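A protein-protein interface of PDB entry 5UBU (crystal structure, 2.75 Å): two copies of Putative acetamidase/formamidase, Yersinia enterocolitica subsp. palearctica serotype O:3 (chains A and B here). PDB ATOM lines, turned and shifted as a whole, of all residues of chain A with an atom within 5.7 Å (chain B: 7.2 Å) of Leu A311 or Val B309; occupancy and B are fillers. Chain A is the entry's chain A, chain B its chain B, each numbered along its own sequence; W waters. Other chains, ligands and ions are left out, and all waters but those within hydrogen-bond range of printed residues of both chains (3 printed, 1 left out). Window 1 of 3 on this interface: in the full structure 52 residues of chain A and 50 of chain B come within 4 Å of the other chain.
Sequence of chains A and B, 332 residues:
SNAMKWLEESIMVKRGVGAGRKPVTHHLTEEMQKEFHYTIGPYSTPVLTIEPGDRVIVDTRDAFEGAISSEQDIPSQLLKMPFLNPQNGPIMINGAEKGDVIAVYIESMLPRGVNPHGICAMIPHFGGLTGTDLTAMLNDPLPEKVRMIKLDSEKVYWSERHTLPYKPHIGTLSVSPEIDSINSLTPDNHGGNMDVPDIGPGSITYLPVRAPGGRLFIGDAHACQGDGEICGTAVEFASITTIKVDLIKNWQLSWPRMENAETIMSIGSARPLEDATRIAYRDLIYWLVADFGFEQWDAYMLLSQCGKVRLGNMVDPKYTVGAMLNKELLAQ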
ATOM      1  N   ASP A 195      -9.223 -14.994   8.276  1.00  0.00           N
ATOM      2  CA  ASP A 195      -9.665 -15.232   9.646  1.00  0.00           C
ATOM      3  C   ASP A 195     -10.594 -14.111  10.142  1.00  0.00           C
ATOM      4  O   ASP A 195     -10.349 -13.484  11.168  1.00  0.00           O
ATOM      5  CB  ASP A 195      -8.470 -15.407  10.588  1.00  0.00           C
ATOM      6  CG  ASP A 195      -7.620 -16.633  10.265  1.00  0.00           C
ATOM      7  OD1 ASP A 195      -8.125 -17.602   9.659  1.00  0.00           O
ATOM      8  OD2 ASP A 195      -6.432 -16.629  10.660  1.00  0.00           O
ATOM      9  N   PRO A 197     -14.202 -13.535  11.507  1.00  0.00           N
ATOM     10  CA  PRO A 197     -15.326 -14.273  12.121  1.00  0.00           C
ATOM     11  C   PRO A 197     -16.673 -14.174  11.408  1.00  0.00           C
ATOM     12  O   PRO A 197     -17.496 -15.081  11.537  1.00  0.00           O
ATOM     13  CB  PRO A 197     -15.454 -13.643  13.500  1.00  0.00           C
ATOM     14  CG  PRO A 197     -14.126 -13.068  13.796  1.00  0.00           C
ATOM     15  CD  PRO A 197     -13.517 -12.671  12.486  1.00  0.00           C
ATOM     16  N   GLN A 225     -14.080 -17.777  17.045  1.00  0.00           N
ATOM     17  CA  GLN A 225     -12.839 -16.987  16.977  1.00  0.00           C
ATOM     18  C   GLN A 225     -13.016 -15.579  17.524  1.00  0.00           C
ATOM     19  O   GLN A 225     -14.015 -14.918  17.255  1.00  0.00           O
ATOM     20  CB  GLN A 225     -12.310 -16.860  15.539  1.00  0.00           C
ATOM     21  CG  GLN A 225     -11.015 -16.070  15.406  1.00  0.00           C
ATOM     22  CD  GLN A 225     -10.657 -15.743  13.978  1.00  0.00           C
ATOM     23  OE1 GLN A 225     -10.611 -16.618  13.121  1.00  0.00           O
ATOM     24  NE2 GLN A 225     -10.356 -14.477  13.727  1.00  0.00           N
ATOM     25  N   GLY A 226     -12.001 -15.116  18.244  1.00  0.00           N
ATOM     26  CA  GLY A 226     -11.995 -13.773  18.787  1.00  0.00           C
ATOM     27  C   GLY A 226     -11.427 -12.794  17.763  1.00  0.00           C
ATOM     28  O   GLY A 226     -10.790 -13.191  16.780  1.00  0.00           O
ATOM     29  N   ASP A 227     -11.662 -11.506  17.993  1.00  0.00           N
ATOM     30  CA  ASP A 227     -11.154 -10.468  17.117  1.00  0.00           C
ATOM     31  C   ASP A 227      -9.638 -10.452  17.280  1.00  0.00           C
ATOM     32  O   ASP A 227      -9.116 -10.234  18.394  1.00  0.00           O
ATOM     33  CB  ASP A 227     -11.737  -9.096  17.481  1.00  0.00           C
ATOM     34  CG  ASP A 227     -13.248  -9.017  17.297  1.00  0.00           C
ATOM     35  OD1 ASP A 227     -13.845  -9.963  16.721  1.00  0.00           O
ATOM     36  OD2 ASP A 227     -13.832  -7.992  17.730  1.00  0.00           O
ATOM     37  N   GLY A 228      -8.942 -10.735  16.179  1.00  0.00           N
ATOM     38  CA  GLY A 228      -7.494 -10.775  16.164  1.00  0.00           C
ATOM     39  C   GLY A 228      -6.903 -12.176  16.216  1.00  0.00           C
ATOM     40  O   GLY A 228      -5.733 -12.341  15.848  1.00  0.00           O
ATOM     41  N   LEU A 273      -0.777  -2.887  10.863  1.00  0.00           N
ATOM     42  CA  LEU A 273      -2.239  -2.983  10.974  1.00  0.00           C
ATOM     43  C   LEU A 273      -2.986  -1.733  10.480  1.00  0.00           C
ATOM     44  O   LEU A 273      -4.113  -1.846  10.021  1.00  0.00           O
ATOM     45  CB  LEU A 273      -2.669  -3.391  12.401  1.00  0.00           C
ATOM     46  CG  LEU A 273      -4.158  -3.747  12.607  1.00  0.00           C
ATOM     47  CD1 LEU A 273      -4.540  -4.976  11.807  1.00  0.00           C
ATOM     48  CD2 LEU A 273      -4.515  -3.949  14.067  1.00  0.00           C
ATOM     49  N   VAL A 309     -15.428  -1.346  12.520  1.00  0.00           N
ATOM     50  CA  VAL A 309     -14.247  -2.110  12.159  1.00  0.00           C
ATOM     51  C   VAL A 309     -14.202  -3.452  12.856  1.00  0.00           C
ATOM     52  O   VAL A 309     -14.506  -3.566  14.047  1.00  0.00           O
ATOM     53  CB  VAL A 309     -12.941  -1.316  12.445  1.00  0.00           C
ATOM     54  CG1 VAL A 309     -11.696  -2.196  12.343  1.00  0.00           C
ATOM     55  CG2 VAL A 309     -12.838  -0.137  11.478  1.00  0.00           C
ATOM     56  N   ARG A 310     -13.840  -4.470  12.081  1.00  0.00           N
ATOM     57  CA  ARG A 310     -13.671  -5.814  12.587  1.00  0.00           C
ATOM     58  C   ARG A 310     -12.211  -6.197  12.422  1.00  0.00           C
ATOM     59  O   ARG A 310     -11.706  -6.241  11.299  1.00  0.00           O
ATOM     60  CB  ARG A 310     -14.518  -6.825  11.823  1.00  0.00           C
ATOM     61  CG  ARG A 310     -14.153  -8.268  12.151  1.00  0.00           C
ATOM     62  CD  ARG A 310     -14.650  -8.702  13.518  1.00  0.00           C
ATOM     63  NE  ARG A 310     -16.068  -9.049  13.460  1.00  0.00           N
ATOM     64  CZ  ARG A 310     -16.816  -9.425  14.501  1.00  0.00           C
ATOM     65  NH1 ARG A 310     -16.316  -9.475  15.744  1.00  0.00           N
ATOM     66  NH2 ARG A 310     -18.081  -9.747  14.299  1.00  0.00           N
ATOM     67  N   LEU A 311     -11.533  -6.453  13.534  1.00  0.00           N
ATOM     68  CA  LEU A 311     -10.180  -6.924  13.472  1.00  0.00           C
ATOM     69  C   LEU A 311     -10.315  -8.433  13.237  1.00  0.00           C
ATOM     70  O   LEU A 311     -10.860  -9.156  14.075  1.00  0.00           O
ATOM     71  CB  LEU A 311      -9.415  -6.631  14.761  1.00  0.00           C
ATOM     72  CG  LEU A 311      -7.993  -7.204  14.829  1.00  0.00           C
ATOM     73  CD1 LEU A 311      -7.159  -6.697  13.666  1.00  0.00           C
ATOM     74  CD2 LEU A 311      -7.335  -6.884  16.156  1.00  0.00           C
ATOM     75  N   GLY A 312      -9.857  -8.894  12.075  1.00  0.00           N
ATOM     76  CA  GLY A 312      -9.912 -10.311  11.727  1.00  0.00           C
ATOM     77  C   GLY A 312      -8.799 -11.037  12.429  1.00  0.00           C
ATOM     78  O   GLY A 312      -8.996 -11.576  13.515  1.00  0.00           O
ATOM     79  N   ASN A 313      -7.620 -11.042  11.816  1.00  0.00           N
ATOM     80  CA  ASN A 313      -6.465 -11.709  12.403  1.00  0.00           C
ATOM     81  C   ASN A 313      -5.372 -10.685  12.602  1.00  0.00           C
ATOM     82  O   ASN A 313      -5.324  -9.668  11.909  1.00  0.00           O
ATOM     83  CB  ASN A 313      -5.973 -12.843  11.487  1.00  0.00           C
ATOM     84  CG  ASN A 313      -5.030 -12.376  10.386  1.00  0.00           C
ATOM     85  OD1 ASN A 313      -3.871 -12.059  10.649  1.00  0.00           O
ATOM     86  ND2 ASN A 313      -5.486 -12.444   9.141  1.00  0.00           N
ATOM     87  N   MET A 314      -4.501 -10.935  13.561  1.00  0.00           N
ATOM     88  CA  MET A 314      -3.372 -10.042  13.770  1.00  0.00           C
ATOM     89  C   MET A 314      -2.200 -10.946  14.072  1.00  0.00           C
ATOM     90  O   MET A 314      -1.298 -10.589  14.812  1.00  0.00           O
ATOM     91  CB  MET A 314      -3.777  -8.898  14.694  1.00  0.00           C
ATOM     92  CG  MET A 314      -3.511  -8.943  16.187  1.00  0.00           C
ATOM     93  SD  MET A 314      -2.588  -7.250  16.636  1.00  0.00           S
ATOM     94  CE  MET A 314      -1.001  -8.108  17.414  1.00  0.00           C
ATOM     95  N   TYR A 319      -2.005  -8.997   8.333  1.00  0.00           N
ATOM     96  CA  TYR A 319      -3.166  -8.861   9.196  1.00  0.00           C
ATOM     97  C   TYR A 319      -4.359  -8.529   8.324  1.00  0.00           C
ATOM     98  O   TYR A 319      -4.195  -8.026   7.231  1.00  0.00           O
ATOM     99  CB  TYR A 319      -2.951  -7.784  10.250  1.00  0.00           C
ATOM    100  CG  TYR A 319      -1.636  -7.892  10.985  1.00  0.00           C
ATOM    101  CD1 TYR A 319      -1.191  -9.105  11.484  1.00  0.00           C
ATOM    102  CD2 TYR A 319      -0.870  -6.758  11.241  1.00  0.00           C
ATOM    103  CE1 TYR A 319      -0.004  -9.197  12.179  1.00  0.00           C
ATOM    104  CE2 TYR A 319       0.310  -6.842  11.934  1.00  0.00           C
ATOM    105  CZ  TYR A 319       0.737  -8.062  12.407  1.00  0.00           C
ATOM    106  OH  TYR A 319       1.911  -8.167  13.111  1.00  0.00           O
ATOM    107  N   THR A 320      -5.555  -8.815   8.817  1.00  0.00           N
ATOM    108  CA  THR A 320      -6.774  -8.572   8.072  1.00  0.00           C
ATOM    109  C   THR A 320      -7.778  -7.780   8.901  1.00  0.00           C
ATOM    110  O   THR A 320      -8.035  -8.100  10.055  1.00  0.00           O
ATOM    111  CB  THR A 320      -7.391  -9.893   7.609  1.00  0.00           C
ATOM    112  OG1 THR A 320      -6.428 -10.606   6.815  1.00  0.00           O
ATOM    113  CG2 THR A 320      -8.663  -9.648   6.795  1.00  0.00           C
ATOM    114  N   VAL A 321      -8.353  -6.759   8.269  1.00  0.00           N
ATOM    115  CA  VAL A 321      -9.310  -5.857   8.882  1.00  0.00           C
ATOM    116  C   VAL A 321     -10.498  -5.649   7.954  1.00  0.00           C
ATOM    117  O   VAL A 321     -10.330  -5.521   6.745  1.00  0.00           O
ATOM    118  CB  VAL A 321      -8.654  -4.481   9.126  1.00  0.00           C
ATOM    119  CG1 VAL A 321      -9.659  -3.485   9.702  1.00  0.00           C
ATOM    120  CG2 VAL A 321      -7.445  -4.618  10.052  1.00  0.00           C
ATOM    121  N   GLY A 322     -11.695  -5.612   8.527  1.00  0.00           N
ATOM    122  CA  GLY A 322     -12.915  -5.396   7.766  1.00  0.00           C
ATOM    123  C   GLY A 322     -13.540  -4.065   8.132  1.00  0.00           C
ATOM    124  O   GLY A 322     -13.732  -3.791   9.306  1.00  0.00           O
ATOM    125  N   ASP B 227     -15.623   3.851  14.104  1.00  0.00           N
ATOM    126  CA  ASP B 227     -14.437   3.152  14.566  1.00  0.00           C
ATOM    127  C   ASP B 227     -13.262   3.667  13.742  1.00  0.00           C
ATOM    128  O   ASP B 227     -13.248   3.540  12.517  1.00  0.00           O
ATOM    129  CB  ASP B 227     -14.594   1.636  14.401  1.00  0.00           C
ATOM    130  CG  ASP B 227     -15.720   1.055  15.254  1.00  0.00           C
ATOM    131  OD1 ASP B 227     -16.274   1.774  16.121  1.00  0.00           O
ATOM    132  OD2 ASP B 227     -16.046  -0.140  15.066  1.00  0.00           O
ATOM    133  N   MET B 265     -12.996  -3.570  29.538  1.00  0.00           N
ATOM    134  CA  MET B 265     -12.093  -3.292  28.433  1.00  0.00           C
ATOM    135  C   MET B 265     -10.805  -2.670  28.860  1.00  0.00           C
ATOM    136  O   MET B 265     -10.785  -1.848  29.761  1.00  0.00           O
ATOM    137  CB  MET B 265     -12.845  -2.317  27.512  1.00  0.00           C
ATOM    138  CG  MET B 265     -12.056  -1.833  26.279  1.00  0.00           C
ATOM    139  SD  MET B 265     -12.835  -0.165  25.525  1.00  0.00           S
ATOM    140  CE  MET B 265     -14.319  -1.037  24.593  1.00  0.00           C
ATOM    141  N   LEU B 273      -0.433   0.459  14.783  1.00  0.00           N
ATOM    142  CA  LEU B 273      -1.702  -0.009  15.354  1.00  0.00           C
ATOM    143  C   LEU B 273      -1.630  -1.402  15.999  1.00  0.00           C
ATOM    144  O   LEU B 273      -2.385  -1.659  16.930  1.00  0.00           O
ATOM    145  CB  LEU B 273      -2.846   0.088  14.323  1.00  0.00           C
ATOM    146  CG  LEU B 273      -4.280  -0.142  14.824  1.00  0.00           C
ATOM    147  CD1 LEU B 273      -4.662   0.933  15.831  1.00  0.00           C
ATOM    148  CD2 LEU B 273      -5.276  -0.150  13.675  1.00  0.00           C
ATOM    149  N   THR B 277      -2.918  -2.611  19.892  1.00  0.00           N
ATOM    150  CA  THR B 277      -3.748  -3.795  20.110  1.00  0.00           C
ATOM    151  C   THR B 277      -3.070  -4.786  21.070  1.00  0.00           C
ATOM    152  O   THR B 277      -3.734  -5.388  21.897  1.00  0.00           O
ATOM    153  CB  THR B 277      -4.070  -4.500  18.791  1.00  0.00           C
ATOM    154  OG1 THR B 277      -4.505  -3.539  17.819  1.00  0.00           O
ATOM    155  CG2 THR B 277      -5.145  -5.568  19.006  1.00  0.00           C
ATOM    156  N   ALA B 280      -3.410  -3.530  24.656  1.00  0.00           N
ATOM    157  CA  ALA B 280      -4.773  -3.729  25.143  1.00  0.00           C
ATOM    158  C   ALA B 280      -5.020  -5.181  25.517  1.00  0.00           C
ATOM    159  O   ALA B 280      -5.438  -5.476  26.651  1.00  0.00           O
ATOM    160  CB  ALA B 280      -5.782  -3.274  24.102  1.00  0.00           C
ATOM    161  N   TYR B 281      -4.775  -6.090  24.576  1.00  0.00           N
ATOM    162  CA  TYR B 281      -4.978  -7.500  24.873  1.00  0.00           C
ATOM    163  C   TYR B 281      -4.130  -8.005  26.025  1.00  0.00           C
ATOM    164  O   TYR B 281      -4.635  -8.737  26.868  1.00  0.00           O
ATOM    165  CB  TYR B 281      -4.810  -8.412  23.656  1.00  0.00           C
ATOM    166  CG  TYR B 281      -6.098  -8.717  22.924  1.00  0.00           C
ATOM    167  CD1 TYR B 281      -7.130  -9.391  23.577  1.00  0.00           C
ATOM    168  CD2 TYR B 281      -6.256  -8.431  21.575  1.00  0.00           C
ATOM    169  CE1 TYR B 281      -8.311  -9.713  22.931  1.00  0.00           C
ATOM    170  CE2 TYR B 281      -7.422  -8.775  20.909  1.00  0.00           C
ATOM    171  CZ  TYR B 281      -8.451  -9.416  21.601  1.00  0.00           C
ATOM    172  OH  TYR B 281      -9.624  -9.743  20.961  1.00  0.00           O
ATOM    173  N   CYS B 306     -12.993 -15.433  22.145  1.00  0.00           N
ATOM    174  CA  CYS B 306     -14.042 -14.511  22.624  1.00  0.00           C
ATOM    175  C   CYS B 306     -13.706 -13.040  22.694  1.00  0.00           C
ATOM    176  O   CYS B 306     -14.589 -12.220  22.951  1.00  0.00           O
ATOM    177  CB  CYS B 306     -14.404 -14.905  24.050  1.00  0.00           C
ATOM    178  SG  CYS B 306     -14.826 -16.626  24.172  1.00  0.00           S
ATOM    179  N   GLY B 307     -12.437 -12.698  22.546  1.00  0.00           N
ATOM    180  CA  GLY B 307     -12.042 -11.309  22.626  1.00  0.00           C
ATOM    181  C   GLY B 307     -12.688 -10.458  21.552  1.00  0.00           C
ATOM    182  O   GLY B 307     -12.890 -10.914  20.430  1.00  0.00           O
ATOM    183  N   LYS B 308     -13.052  -9.240  21.930  1.00  0.00           N
ATOM    184  CA  LYS B 308     -13.635  -8.257  21.019  1.00  0.00           C
ATOM    185  C   LYS B 308     -12.718  -7.045  20.960  1.00  0.00           C
ATOM    186  O   LYS B 308     -12.137  -6.652  21.961  1.00  0.00           O
ATOM    187  CB  LYS B 308     -15.042  -7.805  21.433  1.00  0.00           C
ATOM    188  CG  LYS B 308     -16.161  -8.845  21.459  1.00  0.00           C
ATOM    189  CD  LYS B 308     -16.132  -9.777  20.271  1.00  0.00           C
ATOM    190  CE  LYS B 308     -17.336 -10.710  20.307  1.00  0.00           C
ATOM    191  NZ  LYS B 308     -17.100 -11.763  19.311  1.00  0.00           N
ATOM    192  N   VAL B 309     -12.552  -6.463  19.777  1.00  0.00           N
ATOM    193  CA  VAL B 309     -11.691  -5.296  19.644  1.00  0.00           C
ATOM    194  C   VAL B 309     -12.446  -4.092  19.102  1.00  0.00           C
ATOM    195  O   VAL B 309     -13.257  -4.211  18.174  1.00  0.00           O
ATOM    196  CB  VAL B 309     -10.464  -5.592  18.752  1.00  0.00           C
ATOM    197  CG1 VAL B 309      -9.707  -4.319  18.368  1.00  0.00           C
ATOM    198  CG2 VAL B 309      -9.537  -6.553  19.466  1.00  0.00           C
ATOM    199  N   ARG B 310     -12.176  -2.943  19.720  1.00  0.00           N
ATOM    200  CA  ARG B 310     -12.729  -1.691  19.296  1.00  0.00           C
ATOM    201  C   ARG B 310     -11.627  -0.777  18.844  1.00  0.00           C
ATOM    202  O   ARG B 310     -10.762  -0.436  19.636  1.00  0.00           O
ATOM    203  CB  ARG B 310     -13.548  -1.005  20.399  1.00  0.00           C
ATOM    204  CG  ARG B 310     -13.882   0.449  20.091  1.00  0.00           C
ATOM    205  CD  ARG B 310     -15.318   0.775  20.381  1.00  0.00           C
ATOM    206  NE  ARG B 310     -16.208   0.390  19.292  1.00  0.00           N
ATOM    207  CZ  ARG B 310     -17.537   0.342  19.369  1.00  0.00           C
ATOM    208  NH1 ARG B 310     -18.190   0.587  20.501  1.00  0.00           N
ATOM    209  NH2 ARG B 310     -18.229  -0.019  18.279  1.00  0.00           N
ATOM    210  N   LEU B 311     -11.654  -0.397  17.570  1.00  0.00           N
ATOM    211  CA  LEU B 311     -10.698   0.550  17.068  1.00  0.00           C
ATOM    212  C   LEU B 311     -11.262   1.924  17.464  1.00  0.00           C
ATOM    213  O   LEU B 311     -12.341   2.314  17.018  1.00  0.00           O
ATOM    214  CB  LEU B 311     -10.538   0.431  15.557  1.00  0.00           C
ATOM    215  CG  LEU B 311      -9.625   1.486  14.904  1.00  0.00           C
ATOM    216  CD1 LEU B 311      -8.245   1.424  15.523  1.00  0.00           C
ATOM    217  CD2 LEU B 311      -9.547   1.311  13.403  1.00  0.00           C
ATOM    218  N   GLY B 312     -10.546   2.624  18.335  1.00  0.00           N
ATOM    219  CA  GLY B 312     -10.949   3.948  18.787  1.00  0.00           C
ATOM    220  C   GLY B 312     -10.612   4.963  17.724  1.00  0.00           C
ATOM    221  O   GLY B 312     -11.454   5.291  16.891  1.00  0.00           O
ATOM    222  N   VAL B 321      -6.836   1.549  20.863  1.00  0.00           N
ATOM    223  CA  VAL B 321      -7.574   0.310  20.667  1.00  0.00           C
ATOM    224  C   VAL B 321      -8.049  -0.233  22.009  1.00  0.00           C
ATOM    225  O   VAL B 321      -7.308  -0.195  22.989  1.00  0.00           O
ATOM    226  CB  VAL B 321      -6.650  -0.753  20.031  1.00  0.00           C
ATOM    227  CG1 VAL B 321      -7.373  -2.090  19.883  1.00  0.00           C
ATOM    228  CG2 VAL B 321      -6.118  -0.269  18.682  1.00  0.00           C
ATOM    229  N   GLY B 322      -9.270  -0.754  22.041  1.00  0.00           N
ATOM    230  CA  GLY B 322      -9.838  -1.334  23.253  1.00  0.00           C
ATOM    231  C   GLY B 322     -10.037  -2.834  23.083  1.00  0.00           C
ATOM    232  O   GLY B 322     -10.632  -3.260  22.101  1.00  0.00           O
ATOM    233  N   ALA B 323      -9.523  -3.633  24.017  1.00  0.00           N
ATOM    234  CA  ALA B 323      -9.688  -5.092  23.990  1.00  0.00           C
ATOM    235  C   ALA B 323     -10.750  -5.437  25.029  1.00  0.00           C
ATOM    236  O   ALA B 323     -10.573  -5.162  26.204  1.00  0.00           O
ATOM    237  CB  ALA B 323      -8.378  -5.789  24.308  1.00  0.00           C
ATOM    238  N   MET B 324     -11.843  -6.053  24.593  1.00  0.00           N
ATOM    239  CA  MET B 324     -12.957  -6.378  25.474  1.00  0.00           C
ATOM    240  C   MET B 324     -13.235  -7.816  25.740  1.00  0.00           C
ATOM    241  O   MET B 324     -12.784  -8.691  25.018  1.00  0.00           O
ATOM    242  CB  MET B 324     -14.223  -5.977  24.732  1.00  0.00           C
ATOM    243  CG  MET B 324     -14.641  -4.541  24.950  1.00  0.00           C
ATOM    244  SD  MET B 324     -15.581  -3.985  23.313  1.00  0.00           S
ATOM    245  CE  MET B 324     -17.380  -4.743  23.604  1.00  0.00           C
HETATM  246  O   HOH W   1      -8.723 -12.618  19.536  1.00  0.00           O
HETATM  247  O   HOH W   2     -12.816  -5.886  16.104  1.00  0.00           O
HETATM  248  O   HOH W   3     -14.842 -12.348  17.375  1.00  0.00           O
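Among the printed residues, merely in contact across the chains: Asp A227 with Lys B308, Gly A226 with Gly B307, Leu A273 with Thr B277, Met A314 with Thr B277, Leu A311 with Thr B277, Gly A226 with Cys B306, Leu A273 with Leu B273 and Leu A311 with Val B309.
OD1 of Asp A227 lies within salt-bridge range of NH1 of Arg A310 (2.7 Å).
The backbone NH (N) of Gly A228 lies within hydrogen-bond range of the backbone carbonyl oxygen (O) of Leu A311 (3.3 Å).
The backbone carbonyl oxygen of Gly A228 is in hydrogen-bond range of the backbone NH of Met A314 (3.0 Å).
NH2 of Arg B310 lies within salt-bridge range of OD1 of Asp B227 (3.4 Å).
The side-chain hydroxyl of Thr B277 lies within hydrogen-bond range of the backbone carbonyl oxygen of Leu B273, 3.0 Å away.
The backbone NH (N) of Met B324 sits at hydrogen-bond distance from the backbone carbonyl oxygen (O) of Lys B308.
Of the printed residues of chain B, Leu A311 touches Thr B277 (3.8 Å) and Val B309 (3.99 Å).
Of the printed residues of chain A, Val B309 touches Asp A227 (2.9 Å) and Leu A311 (3.99 Å).
Of the printed residues of chain B, Asp A227 touches Tyr B281 (2.7 Å), Gly B307 (2.8 Å), Lys B308 (3.3 Å) and Val B309 (2.9 Å).
Printed residues of chain B within 4 Å of Gly A226: Cys B306 and Gly B307.
Of the printed residues of chain A, Tyr B281 touches Asp A227 (2.7 Å).
Of the printed residues of chain B, Leu A273 touches Leu B273 (3.9 Å) and Thr B277 (3.8 Å).
Printed residues of chain A within 4 Å of Leu B273: Leu A273 (3.9 Å).
Arg A310 touches none of the printed residues of chain B.
The nearest printed residue of chain B that does not touch Leu A311 is Tyr B281 (5.1 Å).
Of the 17 printed residues of chain B, 8 touch a printed residue of chain A.
Among the printed residues, 12 pairs touch across the chains.
Among the printed residues, no Asp or Glu carboxylate lies within 4 Å of a Lys or Arg side-chain nitrogen of the other chain.
Water W3 lies within hydrogen-bond range of the side-chain carboxylate (OD1) of Asp A227, the backbone carbonyl oxygen (O) of Gln A225 and the side-chain amino group (NZ) of Lys B308.
Water W1 lies within hydrogen-bond range of O of Asp A227, OH of Tyr B281 and O of Gly A226.
Water W2 lies within hydrogen-bond range of the backbone carbonyl oxygen of Val B309 (2.7 Å), the side-chain carboxylate of Asp A227 (2.8 Å) and the backbone NH of Leu A311 (2.9 Å).
Asp A227 touches Val B309, and with the chains exchanged Val A309 touches Asp B227.
Leu A273 touches its own counterpart, Leu B273.
Leu A311 touches Val B309, but with the chains exchanged Val A309 does not touch Leu B311 (4.1 Å).
Of the 12 pairs that touch across the chains among the printed residues, 3 have their exchanged pair printed and touching as well.
O of Asp A227 is in hydrogen-bond range of OH of Tyr B281.
N of Asp A227 is in hydrogen-bond range of O of Gly B307 (2.8 Å).
The backbone NH (N) of Val B309 lies within hydrogen-bond range of the side-chain carboxylate (OD2) of Asp A227.
The side-chain carboxylate (OD2) of Asp B227 is in hydrogen-bond range of the backbone NH (N) of Val A309, 2.9 Å away.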
